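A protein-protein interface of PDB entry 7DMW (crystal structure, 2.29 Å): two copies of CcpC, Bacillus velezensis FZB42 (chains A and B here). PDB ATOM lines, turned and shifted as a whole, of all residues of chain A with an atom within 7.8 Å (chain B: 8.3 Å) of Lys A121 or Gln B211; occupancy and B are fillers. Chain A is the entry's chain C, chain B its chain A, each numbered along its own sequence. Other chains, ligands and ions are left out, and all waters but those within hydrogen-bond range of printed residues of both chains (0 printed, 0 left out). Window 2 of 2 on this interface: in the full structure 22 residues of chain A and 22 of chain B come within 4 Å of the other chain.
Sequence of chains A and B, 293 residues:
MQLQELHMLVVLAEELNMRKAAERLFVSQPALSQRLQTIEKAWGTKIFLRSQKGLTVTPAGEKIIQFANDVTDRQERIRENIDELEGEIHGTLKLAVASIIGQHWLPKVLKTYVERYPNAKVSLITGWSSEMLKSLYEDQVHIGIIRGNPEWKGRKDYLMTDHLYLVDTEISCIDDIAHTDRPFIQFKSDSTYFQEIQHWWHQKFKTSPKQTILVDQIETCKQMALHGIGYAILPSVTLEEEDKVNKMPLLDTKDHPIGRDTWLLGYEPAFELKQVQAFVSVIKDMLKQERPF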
ATOM      1  N   HIS A  90      -3.334   7.423  -7.392  1.00  0.00           N
ATOM      2  CA  HIS A  90      -4.372   7.085  -8.358  1.00  0.00           C
ATOM      3  C   HIS A  90      -4.465   5.574  -8.568  1.00  0.00           C
ATOM      4  O   HIS A  90      -3.794   4.806  -7.883  1.00  0.00           O
ATOM      5  CB  HIS A  90      -4.122   7.793  -9.688  1.00  0.00           C
ATOM      6  CG  HIS A  90      -2.731   7.625 -10.222  1.00  0.00           C
ATOM      7  ND1 HIS A  90      -2.478   7.128 -11.484  1.00  0.00           N
ATOM      8  CD2 HIS A  90      -1.522   7.913  -9.682  1.00  0.00           C
ATOM      9  CE1 HIS A  90      -1.172   7.098 -11.691  1.00  0.00           C
ATOM     10  NE2 HIS A  90      -0.569   7.572 -10.615  1.00  0.00           N
ATOM     11  N   GLY A  91      -5.294   5.156  -9.523  1.00  0.00           N
ATOM     12  CA  GLY A  91      -5.652   3.754  -9.668  1.00  0.00           C
ATOM     13  C   GLY A  91      -4.468   2.840  -9.966  1.00  0.00           C
ATOM     14  O   GLY A  91      -3.338   3.259 -10.232  1.00  0.00           O
ATOM     15  N   THR A  92      -4.764   1.541  -9.919  1.00  0.00           N
ATOM     16  CA  THR A  92      -3.763   0.491 -10.059  1.00  0.00           C
ATOM     17  C   THR A  92      -3.729   0.039 -11.508  1.00  0.00           C
ATOM     18  O   THR A  92      -4.761  -0.371 -12.056  1.00  0.00           O
ATOM     19  CB  THR A  92      -4.075  -0.710  -9.158  1.00  0.00           C
ATOM     20  OG1 THR A  92      -5.458  -1.062  -9.297  1.00  0.00           O
ATOM     21  CG2 THR A  92      -3.807  -0.377  -7.699  1.00  0.00           C
ATOM     22  N   LEU A  93      -2.546   0.089 -12.116  1.00  0.00           N
ATOM     23  CA  LEU A  93      -2.376  -0.251 -13.523  1.00  0.00           C
ATOM     24  C   LEU A  93      -2.098  -1.744 -13.660  1.00  0.00           C
ATOM     25  O   LEU A  93      -1.083  -2.236 -13.155  1.00  0.00           O
ATOM     26  CB  LEU A  93      -1.233   0.574 -14.105  1.00  0.00           C
ATOM     27  CG  LEU A  93      -0.733   0.241 -15.507  1.00  0.00           C
ATOM     28  CD1 LEU A  93      -1.834   0.447 -16.534  1.00  0.00           C
ATOM     29  CD2 LEU A  93       0.467   1.109 -15.821  1.00  0.00           C
ATOM     30  N   LYS A  94      -2.985  -2.464 -14.338  1.00  0.00           N
ATOM     31  CA  LYS A  94      -2.825  -3.905 -14.530  1.00  0.00           C
ATOM     32  C   LYS A  94      -2.229  -4.169 -15.912  1.00  0.00           C
ATOM     33  O   LYS A  94      -2.943  -4.145 -16.917  1.00  0.00           O
ATOM     34  CB  LYS A  94      -4.161  -4.625 -14.375  1.00  0.00           C
ATOM     35  CG  LYS A  94      -4.889  -4.356 -13.073  1.00  0.00           C
ATOM     36  CD  LYS A  94      -6.135  -5.235 -12.986  1.00  0.00           C
ATOM     37  CE  LYS A  94      -7.333  -4.445 -12.451  1.00  0.00           C
ATOM     38  NZ  LYS A  94      -7.149  -4.017 -11.027  1.00  0.00           N
ATOM     39  N   LEU A  95      -0.932  -4.466 -15.960  1.00  0.00           N
ATOM     40  CA  LEU A  95      -0.228  -4.703 -17.211  1.00  0.00           C
ATOM     41  C   LEU A  95      -0.091  -6.189 -17.545  1.00  0.00           C
ATOM     42  O   LEU A  95       0.052  -7.045 -16.663  1.00  0.00           O
ATOM     43  CB  LEU A  95       1.166  -4.083 -17.165  1.00  0.00           C
ATOM     44  CG  LEU A  95       1.273  -2.591 -16.886  1.00  0.00           C
ATOM     45  CD1 LEU A  95       2.705  -2.240 -16.574  1.00  0.00           C
ATOM     46  CD2 LEU A  95       0.747  -1.777 -18.107  1.00  0.00           C
ATOM     47  N   LEU A 110       9.079   1.471 -16.370  1.00  0.00           N
ATOM     48  CA  LEU A 110       8.439   1.487 -15.057  1.00  0.00           C
ATOM     49  C   LEU A 110       9.199   2.351 -14.063  1.00  0.00           C
ATOM     50  O   LEU A 110       8.582   3.010 -13.221  1.00  0.00           O
ATOM     51  CB  LEU A 110       8.300   0.064 -14.519  1.00  0.00           C
ATOM     52  CG  LEU A 110       6.899  -0.532 -14.643  1.00  0.00           C
ATOM     53  CD1 LEU A 110       6.846  -1.947 -14.073  1.00  0.00           C
ATOM     54  CD2 LEU A 110       5.901   0.360 -13.945  1.00  0.00           C
ATOM     55  N   TYR A 113       7.942   5.677 -14.611  1.00  0.00           N
ATOM     56  CA  TYR A 113       6.553   5.816 -14.179  1.00  0.00           C
ATOM     57  C   TYR A 113       6.425   5.898 -12.659  1.00  0.00           C
ATOM     58  O   TYR A 113       5.552   6.615 -12.158  1.00  0.00           O
ATOM     59  CB  TYR A 113       5.726   4.658 -14.722  1.00  0.00           C
ATOM     60  CG  TYR A 113       4.277   4.642 -14.295  1.00  0.00           C
ATOM     61  CD1 TYR A 113       3.330   5.425 -14.954  1.00  0.00           C
ATOM     62  CD2 TYR A 113       3.839   3.812 -13.261  1.00  0.00           C
ATOM     63  CE1 TYR A 113       1.987   5.394 -14.583  1.00  0.00           C
ATOM     64  CE2 TYR A 113       2.506   3.774 -12.888  1.00  0.00           C
ATOM     65  CZ  TYR A 113       1.583   4.572 -13.545  1.00  0.00           C
ATOM     66  OH  TYR A 113       0.259   4.542 -13.175  1.00  0.00           O
ATOM     67  N   VAL A 114       7.258   5.161 -11.915  1.00  0.00           N
ATOM     68  CA  VAL A 114       7.262   5.284 -10.459  1.00  0.00           C
ATOM     69  C   VAL A 114       7.938   6.582 -10.048  1.00  0.00           C
ATOM     70  O   VAL A 114       7.564   7.193  -9.039  1.00  0.00           O
ATOM     71  CB  VAL A 114       7.948   4.067  -9.795  1.00  0.00           C
ATOM     72  CG1 VAL A 114       8.066   4.278  -8.298  1.00  0.00           C
ATOM     73  CG2 VAL A 114       7.173   2.780 -10.061  1.00  0.00           C
ATOM     74  N   TYR A 117       5.363   9.229 -10.351  1.00  0.00           N
ATOM     75  CA  TYR A 117       4.081   8.906  -9.728  1.00  0.00           C
ATOM     76  C   TYR A 117       4.303   8.001  -8.525  1.00  0.00           C
ATOM     77  O   TYR A 117       3.973   6.809  -8.551  1.00  0.00           O
ATOM     78  CB  TYR A 117       3.140   8.256 -10.738  1.00  0.00           C
ATOM     79  CG  TYR A 117       2.824   9.144 -11.908  1.00  0.00           C
ATOM     80  CD1 TYR A 117       1.879  10.149 -11.798  1.00  0.00           C
ATOM     81  CD2 TYR A 117       3.464   8.972 -13.131  1.00  0.00           C
ATOM     82  CE1 TYR A 117       1.578  10.958 -12.869  1.00  0.00           C
ATOM     83  CE2 TYR A 117       3.169   9.773 -14.205  1.00  0.00           C
ATOM     84  CZ  TYR A 117       2.224  10.769 -14.069  1.00  0.00           C
ATOM     85  OH  TYR A 117       1.927  11.581 -15.139  1.00  0.00           O
ATOM     86  N   PRO A 118       4.845   8.549  -7.436  1.00  0.00           N
ATOM     87  CA  PRO A 118       5.038   7.742  -6.231  1.00  0.00           C
ATOM     88  C   PRO A 118       3.697   7.269  -5.703  1.00  0.00           C
ATOM     89  O   PRO A 118       2.664   7.907  -5.920  1.00  0.00           O
ATOM     90  CB  PRO A 118       5.719   8.711  -5.255  1.00  0.00           C
ATOM     91  CG  PRO A 118       6.232   9.835  -6.098  1.00  0.00           C
ATOM     92  CD  PRO A 118       5.262   9.948  -7.230  1.00  0.00           C
ATOM     93  N   ASN A 119       3.721   6.124  -5.024  1.00  0.00           N
ATOM     94  CA  ASN A 119       2.536   5.516  -4.417  1.00  0.00           C
ATOM     95  C   ASN A 119       1.508   5.096  -5.460  1.00  0.00           C
ATOM     96  O   ASN A 119       0.337   4.875  -5.133  1.00  0.00           O
ATOM     97  CB  ASN A 119       1.877   6.448  -3.394  1.00  0.00           C
ATOM     98  CG  ASN A 119       2.879   7.139  -2.505  1.00  0.00           C
ATOM     99  OD1 ASN A 119       2.625   8.247  -2.024  1.00  0.00           O
ATOM    100  ND2 ASN A 119       4.022   6.490  -2.261  1.00  0.00           N
ATOM    101  N   ALA A 120       1.919   5.002  -6.717  1.00  0.00           N
ATOM    102  CA  ALA A 120       1.051   4.500  -7.768  1.00  0.00           C
ATOM    103  C   ALA A 120       1.334   3.014  -7.922  1.00  0.00           C
ATOM    104  O   ALA A 120       2.484   2.615  -8.141  1.00  0.00           O
ATOM    105  CB  ALA A 120       1.281   5.253  -9.077  1.00  0.00           C
ATOM    106  N   LYS A 121       0.300   2.200  -7.780  1.00  0.00           N
ATOM    107  CA  LYS A 121       0.502   0.768  -7.781  1.00  0.00           C
ATOM    108  C   LYS A 121       0.534   0.225  -9.204  1.00  0.00           C
ATOM    109  O   LYS A 121      -0.147   0.730 -10.104  1.00  0.00           O
ATOM    110  CB  LYS A 121      -0.592   0.083  -6.967  1.00  0.00           C
ATOM    111  CG  LYS A 121      -0.802   0.648  -5.554  1.00  0.00           C
ATOM    112  CD  LYS A 121      -1.866  -0.165  -4.807  1.00  0.00           C
ATOM    113  CE  LYS A 121      -2.370   0.534  -3.545  1.00  0.00           C
ATOM    114  NZ  LYS A 121      -1.565   0.171  -2.335  1.00  0.00           N
ATOM    115  N   VAL A 122       1.354  -0.813  -9.403  1.00  0.00           N
ATOM    116  CA  VAL A 122       1.461  -1.500 -10.683  1.00  0.00           C
ATOM    117  C   VAL A 122       1.335  -2.997 -10.432  1.00  0.00           C
ATOM    118  O   VAL A 122       1.834  -3.514  -9.427  1.00  0.00           O
ATOM    119  CB  VAL A 122       2.795  -1.176 -11.391  1.00  0.00           C
ATOM    120  CG1 VAL A 122       2.842  -1.815 -12.758  1.00  0.00           C
ATOM    121  CG2 VAL A 122       3.023   0.322 -11.481  1.00  0.00           C
ATOM    122  N   SER A 123       0.682  -3.696 -11.349  1.00  0.00           N
ATOM    123  CA  SER A 123       0.485  -5.129 -11.215  1.00  0.00           C
ATOM    124  C   SER A 123       0.757  -5.770 -12.566  1.00  0.00           C
ATOM    125  O   SER A 123       0.127  -5.401 -13.562  1.00  0.00           O
ATOM    126  CB  SER A 123      -0.931  -5.424 -10.720  1.00  0.00           C
ATOM    127  OG  SER A 123      -1.407  -6.642 -11.236  1.00  0.00           O
ATOM    128  N   HIS A 142      -5.549  -3.890 -17.954  1.00  0.00           N
ATOM    129  CA  HIS A 142      -5.847  -2.673 -18.705  1.00  0.00           C
ATOM    130  C   HIS A 142      -5.211  -2.680 -20.094  1.00  0.00           C
ATOM    131  O   HIS A 142      -5.865  -2.355 -21.091  1.00  0.00           O
ATOM    132  CB  HIS A 142      -5.344  -1.460 -17.933  1.00  0.00           C
ATOM    133  CG  HIS A 142      -6.056  -1.230 -16.647  1.00  0.00           C
ATOM    134  ND1 HIS A 142      -5.433  -0.704 -15.536  1.00  0.00           N
ATOM    135  CD2 HIS A 142      -7.345  -1.450 -16.292  1.00  0.00           C
ATOM    136  CE1 HIS A 142      -6.310  -0.603 -14.552  1.00  0.00           C
ATOM    137  NE2 HIS A 142      -7.478  -1.046 -14.987  1.00  0.00           N
ATOM    138  N   GLN A 275      -4.485   6.308 -14.850  1.00  0.00           N
ATOM    139  CA  GLN A 275      -3.140   5.753 -14.750  1.00  0.00           C
ATOM    140  C   GLN A 275      -2.700   5.143 -16.073  1.00  0.00           C
ATOM    141  O   GLN A 275      -1.509   5.165 -16.395  1.00  0.00           O
ATOM    142  CB  GLN A 275      -3.057   4.716 -13.623  1.00  0.00           C
ATOM    143  CG  GLN A 275      -3.822   3.433 -13.879  1.00  0.00           C
ATOM    144  CD  GLN A 275      -5.300   3.558 -13.551  1.00  0.00           C
ATOM    145  OE1 GLN A 275      -5.850   4.668 -13.500  1.00  0.00           O
ATOM    146  NE2 GLN A 275      -5.959   2.423 -13.356  1.00  0.00           N
ATOM    147  N   PRO B 183       9.213   1.546  -3.097  1.00  0.00           N
ATOM    148  CA  PRO B 183       8.172   0.516  -3.150  1.00  0.00           C
ATOM    149  C   PRO B 183       8.749  -0.875  -2.932  1.00  0.00           C
ATOM    150  O   PRO B 183       9.922  -1.159  -3.204  1.00  0.00           O
ATOM    151  CB  PRO B 183       7.589   0.674  -4.557  1.00  0.00           C
ATOM    152  CG  PRO B 183       8.735   1.229  -5.370  1.00  0.00           C
ATOM    153  CD  PRO B 183       9.599   2.031  -4.434  1.00  0.00           C
ATOM    154  N   PHE B 184       7.909  -1.737  -2.381  1.00  0.00           N
ATOM    155  CA  PHE B 184       8.219  -3.154  -2.267  1.00  0.00           C
ATOM    156  C   PHE B 184       7.823  -3.790  -3.595  1.00  0.00           C
ATOM    157  O   PHE B 184       6.636  -3.982  -3.885  1.00  0.00           O
ATOM    158  CB  PHE B 184       7.478  -3.756  -1.078  1.00  0.00           C
ATOM    159  CG  PHE B 184       7.729  -5.226  -0.865  1.00  0.00           C
ATOM    160  CD1 PHE B 184       8.709  -5.901  -1.569  1.00  0.00           C
ATOM    161  CD2 PHE B 184       6.967  -5.932   0.049  1.00  0.00           C
ATOM    162  CE1 PHE B 184       8.913  -7.237  -1.384  1.00  0.00           C
ATOM    163  CE2 PHE B 184       7.167  -7.274   0.255  1.00  0.00           C
ATOM    164  CZ  PHE B 184       8.144  -7.932  -0.463  1.00  0.00           C
ATOM    165  N   ILE B 185       8.813  -4.082  -4.432  1.00  0.00           N
ATOM    166  CA  ILE B 185       8.555  -4.918  -5.597  1.00  0.00           C
ATOM    167  C   ILE B 185       8.495  -6.347  -5.095  1.00  0.00           C
ATOM    168  O   ILE B 185       9.435  -6.827  -4.463  1.00  0.00           O
ATOM    169  CB  ILE B 185       9.628  -4.756  -6.678  1.00  0.00           C
ATOM    170  CG1 ILE B 185       9.937  -3.283  -6.924  1.00  0.00           C
ATOM    171  CG2 ILE B 185       9.169  -5.448  -7.951  1.00  0.00           C
ATOM    172  CD1 ILE B 185      11.363  -3.047  -7.271  1.00  0.00           C
ATOM    173  N   GLN B 186       7.413  -7.035  -5.415  1.00  0.00           N
ATOM    174  CA  GLN B 186       6.976  -8.201  -4.682  1.00  0.00           C
ATOM    175  C   GLN B 186       6.548  -9.265  -5.679  1.00  0.00           C
ATOM    176  O   GLN B 186       5.630  -9.038  -6.477  1.00  0.00           O
ATOM    177  CB  GLN B 186       5.828  -7.796  -3.767  1.00  0.00           C
ATOM    178  CG  GLN B 186       5.129  -8.905  -3.073  1.00  0.00           C
ATOM    179  CD  GLN B 186       4.620  -8.465  -1.709  1.00  0.00           C
ATOM    180  OE1 GLN B 186       4.018  -7.396  -1.571  1.00  0.00           O
ATOM    181  NE2 GLN B 186       4.872  -9.285  -0.692  1.00  0.00           N
ATOM    182  N   PHE B 187       7.224 -10.413  -5.655  1.00  0.00           N
ATOM    183  CA  PHE B 187       6.818 -11.527  -6.501  1.00  0.00           C
ATOM    184  C   PHE B 187       5.626 -12.234  -5.873  1.00  0.00           C
ATOM    185  O   PHE B 187       5.529 -12.350  -4.648  1.00  0.00           O
ATOM    186  CB  PHE B 187       7.985 -12.499  -6.701  1.00  0.00           C
ATOM    187  CG  PHE B 187       7.585 -13.859  -7.253  1.00  0.00           C
ATOM    188  CD1 PHE B 187       7.466 -14.062  -8.629  1.00  0.00           C
ATOM    189  CD2 PHE B 187       7.368 -14.947  -6.397  1.00  0.00           C
ATOM    190  CE1 PHE B 187       7.114 -15.305  -9.144  1.00  0.00           C
ATOM    191  CE2 PHE B 187       7.006 -16.202  -6.905  1.00  0.00           C
ATOM    192  CZ  PHE B 187       6.888 -16.385  -8.273  1.00  0.00           C
ATOM    193  N   LYS B 188       4.709 -12.707  -6.714  1.00  0.00           N
ATOM    194  CA  LYS B 188       3.601 -13.517  -6.216  1.00  0.00           C
ATOM    195  C   LYS B 188       3.190 -14.543  -7.253  1.00  0.00           C
ATOM    196  O   LYS B 188       2.790 -14.182  -8.361  1.00  0.00           O
ATOM    197  CB  LYS B 188       2.392 -12.668  -5.843  1.00  0.00           C
ATOM    198  CG  LYS B 188       1.107 -13.485  -5.768  1.00  0.00           C
ATOM    199  CD  LYS B 188       0.074 -12.816  -4.880  1.00  0.00           C
ATOM    200  CE  LYS B 188      -1.000 -13.807  -4.456  1.00  0.00           C
ATOM    201  NZ  LYS B 188      -2.096 -13.077  -3.770  1.00  0.00           N
ATOM    202  N   PHE B 194       5.251 -16.299  -1.525  1.00  0.00           N
ATOM    203  CA  PHE B 194       4.682 -15.008  -1.178  1.00  0.00           C
ATOM    204  C   PHE B 194       4.211 -15.013   0.270  1.00  0.00           C
ATOM    205  O   PHE B 194       4.560 -14.120   1.049  1.00  0.00           O
ATOM    206  CB  PHE B 194       3.543 -14.665  -2.154  1.00  0.00           C
ATOM    207  CG  PHE B 194       2.819 -13.392  -1.820  1.00  0.00           C
ATOM    208  CD1 PHE B 194       3.284 -12.175  -2.279  1.00  0.00           C
ATOM    209  CD2 PHE B 194       1.679 -13.412  -1.032  1.00  0.00           C
ATOM    210  CE1 PHE B 194       2.625 -11.004  -1.968  1.00  0.00           C
ATOM    211  CE2 PHE B 194       1.022 -12.249  -0.714  1.00  0.00           C
ATOM    212  CZ  PHE B 194       1.497 -11.041  -1.192  1.00  0.00           C
ATOM    213  N   GLN B 198       5.392 -12.682   3.543  1.00  0.00           N
ATOM    214  CA  GLN B 198       4.419 -11.943   4.341  1.00  0.00           C
ATOM    215  C   GLN B 198       4.571 -12.291   5.819  1.00  0.00           C
ATOM    216  O   GLN B 198       4.679 -11.404   6.675  1.00  0.00           O
ATOM    217  CB  GLN B 198       3.004 -12.254   3.865  1.00  0.00           C
ATOM    218  CG  GLN B 198       2.755 -11.895   2.419  1.00  0.00           C
ATOM    219  CD  GLN B 198       2.831 -10.413   2.187  1.00  0.00           C
ATOM    220  OE1 GLN B 198       3.817  -9.912   1.644  1.00  0.00           O
ATOM    221  NE2 GLN B 198       1.805  -9.692   2.624  1.00  0.00           N
ATOM    222  N   SER B 208       2.315  -4.224   8.185  1.00  0.00           N
ATOM    223  CA  SER B 208       2.088  -4.884   6.910  1.00  0.00           C
ATOM    224  C   SER B 208       2.915  -4.204   5.824  1.00  0.00           C
ATOM    225  O   SER B 208       3.334  -3.052   5.977  1.00  0.00           O
ATOM    226  CB  SER B 208       0.600  -4.864   6.537  1.00  0.00           C
ATOM    227  OG  SER B 208       0.252  -6.015   5.783  1.00  0.00           O
ATOM    228  N   PRO B 209       3.218  -4.899   4.736  1.00  0.00           N
ATOM    229  CA  PRO B 209       4.032  -4.297   3.680  1.00  0.00           C
ATOM    230  C   PRO B 209       3.168  -3.651   2.596  1.00  0.00           C
ATOM    231  O   PRO B 209       1.960  -3.895   2.490  1.00  0.00           O
ATOM    232  CB  PRO B 209       4.809  -5.503   3.139  1.00  0.00           C
ATOM    233  CG  PRO B 209       3.794  -6.635   3.259  1.00  0.00           C
ATOM    234  CD  PRO B 209       2.923  -6.318   4.462  1.00  0.00           C
ATOM    235  N   LYS B 210       3.825  -2.826   1.775  1.00  0.00           N
ATOM    236  CA  LYS B 210       3.149  -1.932   0.826  1.00  0.00           C
ATOM    237  C   LYS B 210       2.910  -2.633  -0.511  1.00  0.00           C
ATOM    238  O   LYS B 210       3.774  -2.630  -1.396  1.00  0.00           O
ATOM    239  CB  LYS B 210       3.961  -0.653   0.626  1.00  0.00           C
ATOM    240  CG  LYS B 210       4.467   0.015   1.924  1.00  0.00           C
ATOM    241  CD  LYS B 210       3.366   0.232   2.992  1.00  0.00           C
ATOM    242  CE  LYS B 210       2.064   0.832   2.424  1.00  0.00           C
ATOM    243  NZ  LYS B 210       0.932   0.762   3.421  1.00  0.00           N
ATOM    244  N   GLN B 211       1.704  -3.183  -0.678  1.00  0.00           N
ATOM    245  CA  GLN B 211       1.275  -3.811  -1.928  1.00  0.00           C
ATOM    246  C   GLN B 211       1.111  -2.741  -3.007  1.00  0.00           C
ATOM    247  O   GLN B 211       0.001  -2.310  -3.341  1.00  0.00           O
ATOM    248  CB  GLN B 211      -0.028  -4.576  -1.713  1.00  0.00           C
ATOM    249  CG  GLN B 211      -0.330  -5.652  -2.760  1.00  0.00           C
ATOM    250  CD  GLN B 211      -0.284  -7.067  -2.182  1.00  0.00           C
ATOM    251  OE1 GLN B 211       0.417  -7.332  -1.189  1.00  0.00           O
ATOM    252  NE2 GLN B 211      -1.033  -7.985  -2.802  1.00  0.00           N
ATOM    253  N   THR B 212       2.244  -2.295  -3.558  1.00  0.00           N
ATOM    254  CA  THR B 212       2.241  -1.402  -4.709  1.00  0.00           C
ATOM    255  C   THR B 212       2.564  -2.156  -5.996  1.00  0.00           C
ATOM    256  O   THR B 212       1.714  -2.260  -6.888  1.00  0.00           O
ATOM    257  CB  THR B 212       3.213  -0.231  -4.492  1.00  0.00           C
ATOM    258  OG1 THR B 212       4.536  -0.595  -4.906  1.00  0.00           O
ATOM    259  CG2 THR B 212       3.224   0.184  -3.030  1.00  0.00           C
ATOM    260  N   ILE B 213       3.765  -2.720  -6.099  1.00  0.00           N
ATOM    261  CA  ILE B 213       4.186  -3.425  -7.305  1.00  0.00           C
ATOM    262  C   ILE B 213       4.136  -4.933  -7.063  1.00  0.00           C
ATOM    263  O   ILE B 213       4.832  -5.465  -6.185  1.00  0.00           O
ATOM    264  CB  ILE B 213       5.583  -2.982  -7.752  1.00  0.00           C
ATOM    265  CG1 ILE B 213       5.632  -1.458  -7.879  1.00  0.00           C
ATOM    266  CG2 ILE B 213       5.923  -3.656  -9.062  1.00  0.00           C
ATOM    267  CD1 ILE B 213       6.859  -0.935  -8.588  1.00  0.00           C
ATOM    268  N   LEU B 214       3.332  -5.612  -7.878  1.00  0.00           N
ATOM    269  CA  LEU B 214       3.122  -7.048  -7.826  1.00  0.00           C
ATOM    270  C   LEU B 214       3.542  -7.651  -9.163  1.00  0.00           C
ATOM    271  O   LEU B 214       3.014  -7.271 -10.213  1.00  0.00           O
ATOM    272  CB  LEU B 214       1.653  -7.346  -7.528  1.00  0.00           C
ATOM    273  CG  LEU B 214       1.305  -8.694  -6.908  1.00  0.00           C
ATOM    274  CD1 LEU B 214       1.949  -8.804  -5.547  1.00  0.00           C
ATOM    275  CD2 LEU B 214      -0.195  -8.808  -6.785  1.00  0.00           C
ATOM    276  N   TYR B 231      12.968  -2.119  -3.633  1.00  0.00           N
ATOM    277  CA  TYR B 231      13.627  -3.279  -3.053  1.00  0.00           C
ATOM    278  C   TYR B 231      12.828  -4.545  -3.331  1.00  0.00           C
ATOM    279  O   TYR B 231      11.634  -4.507  -3.655  1.00  0.00           O
ATOM    280  CB  TYR B 231      13.847  -3.119  -1.537  1.00  0.00           C
ATOM    281  CG  TYR B 231      12.571  -2.992  -0.739  1.00  0.00           C
ATOM    282  CD1 TYR B 231      11.917  -4.115  -0.247  1.00  0.00           C
ATOM    283  CD2 TYR B 231      12.032  -1.743  -0.462  1.00  0.00           C
ATOM    284  CE1 TYR B 231      10.751  -3.998   0.482  1.00  0.00           C
ATOM    285  CE2 TYR B 231      10.865  -1.613   0.267  1.00  0.00           C
ATOM    286  CZ  TYR B 231      10.225  -2.740   0.734  1.00  0.00           C
ATOM    287  OH  TYR B 231       9.061  -2.597   1.461  1.00  0.00           O
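No position is printed for both chains.
The backbone carbonyl oxygen (O) of Gln B211 sits at hydrogen-bond distance from the side-chain amino group (NZ) of Lys A121 (3.1 Å).
O of Val A122 lies within hydrogen-bond range of N of Leu B214 (3.0 Å).
The backbone carbonyl oxygen of Thr B212 is in hydrogen-bond range of the backbone NH of Val A122, at 2.9 Å.
Of the printed residues of chain B, Lys A121 touches Gln B211 and Thr B212.
Printed residues of chain B within 4 Å of Val A122: Thr B212, Ile B213 and Leu B214.
Of the printed residues of chain B, Ser A123 touches Leu B214.
Gln B211 touches just one residue of chain A: Lys A121.
Printed residues of chain A within 4 Å of Thr B212: Lys A121 and Val A122.
Of the printed residues of chain A, Ile B213 touches Val A122.
Of the printed residues of chain A, Leu B214 touches Val A122 and Ser A123.
The nearest residue of chain A that does not touch Gln B211 is Thr A92 (6.1 Å).
The nearest printed residue of chain B that does not touch Ser A123 is Thr B212 (4.8 Å).
Lys A121 touches Thr B212.
Ile B213 touches Val A122.
O of Leu B214 touches CA of Ser A123, 3.5 Å away.
O of Lys A121 is in hydrogen-bond range of N of Leu A93 (3.2 Å).
N of Ser A123 is in hydrogen-bond range of O of Leu A93 (2.9 Å).
The backbone carbonyl oxygen (O) of Ser A123 lies within hydrogen-bond range of the backbone NH (N) of Leu A95 (2.8 Å).
The backbone carbonyl oxygen (O) of Ile B213 sits at hydrogen-bond distance from the backbone NH (N) of Gln B186 (3.1 Å).
Of the 16 printed residues of chain B, 4 touch a printed residue of chain A.
Printed residues of chain A that touch a printed residue of chain B: Lys A121, Val A122 and Ser A123.
Among the printed residues, 6 pairs touch across the chains.
Among the printed residues, no Asp or Glu carboxylate lies within 4 Å of a Lys or Arg side-chain nitrogen of the other chain.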
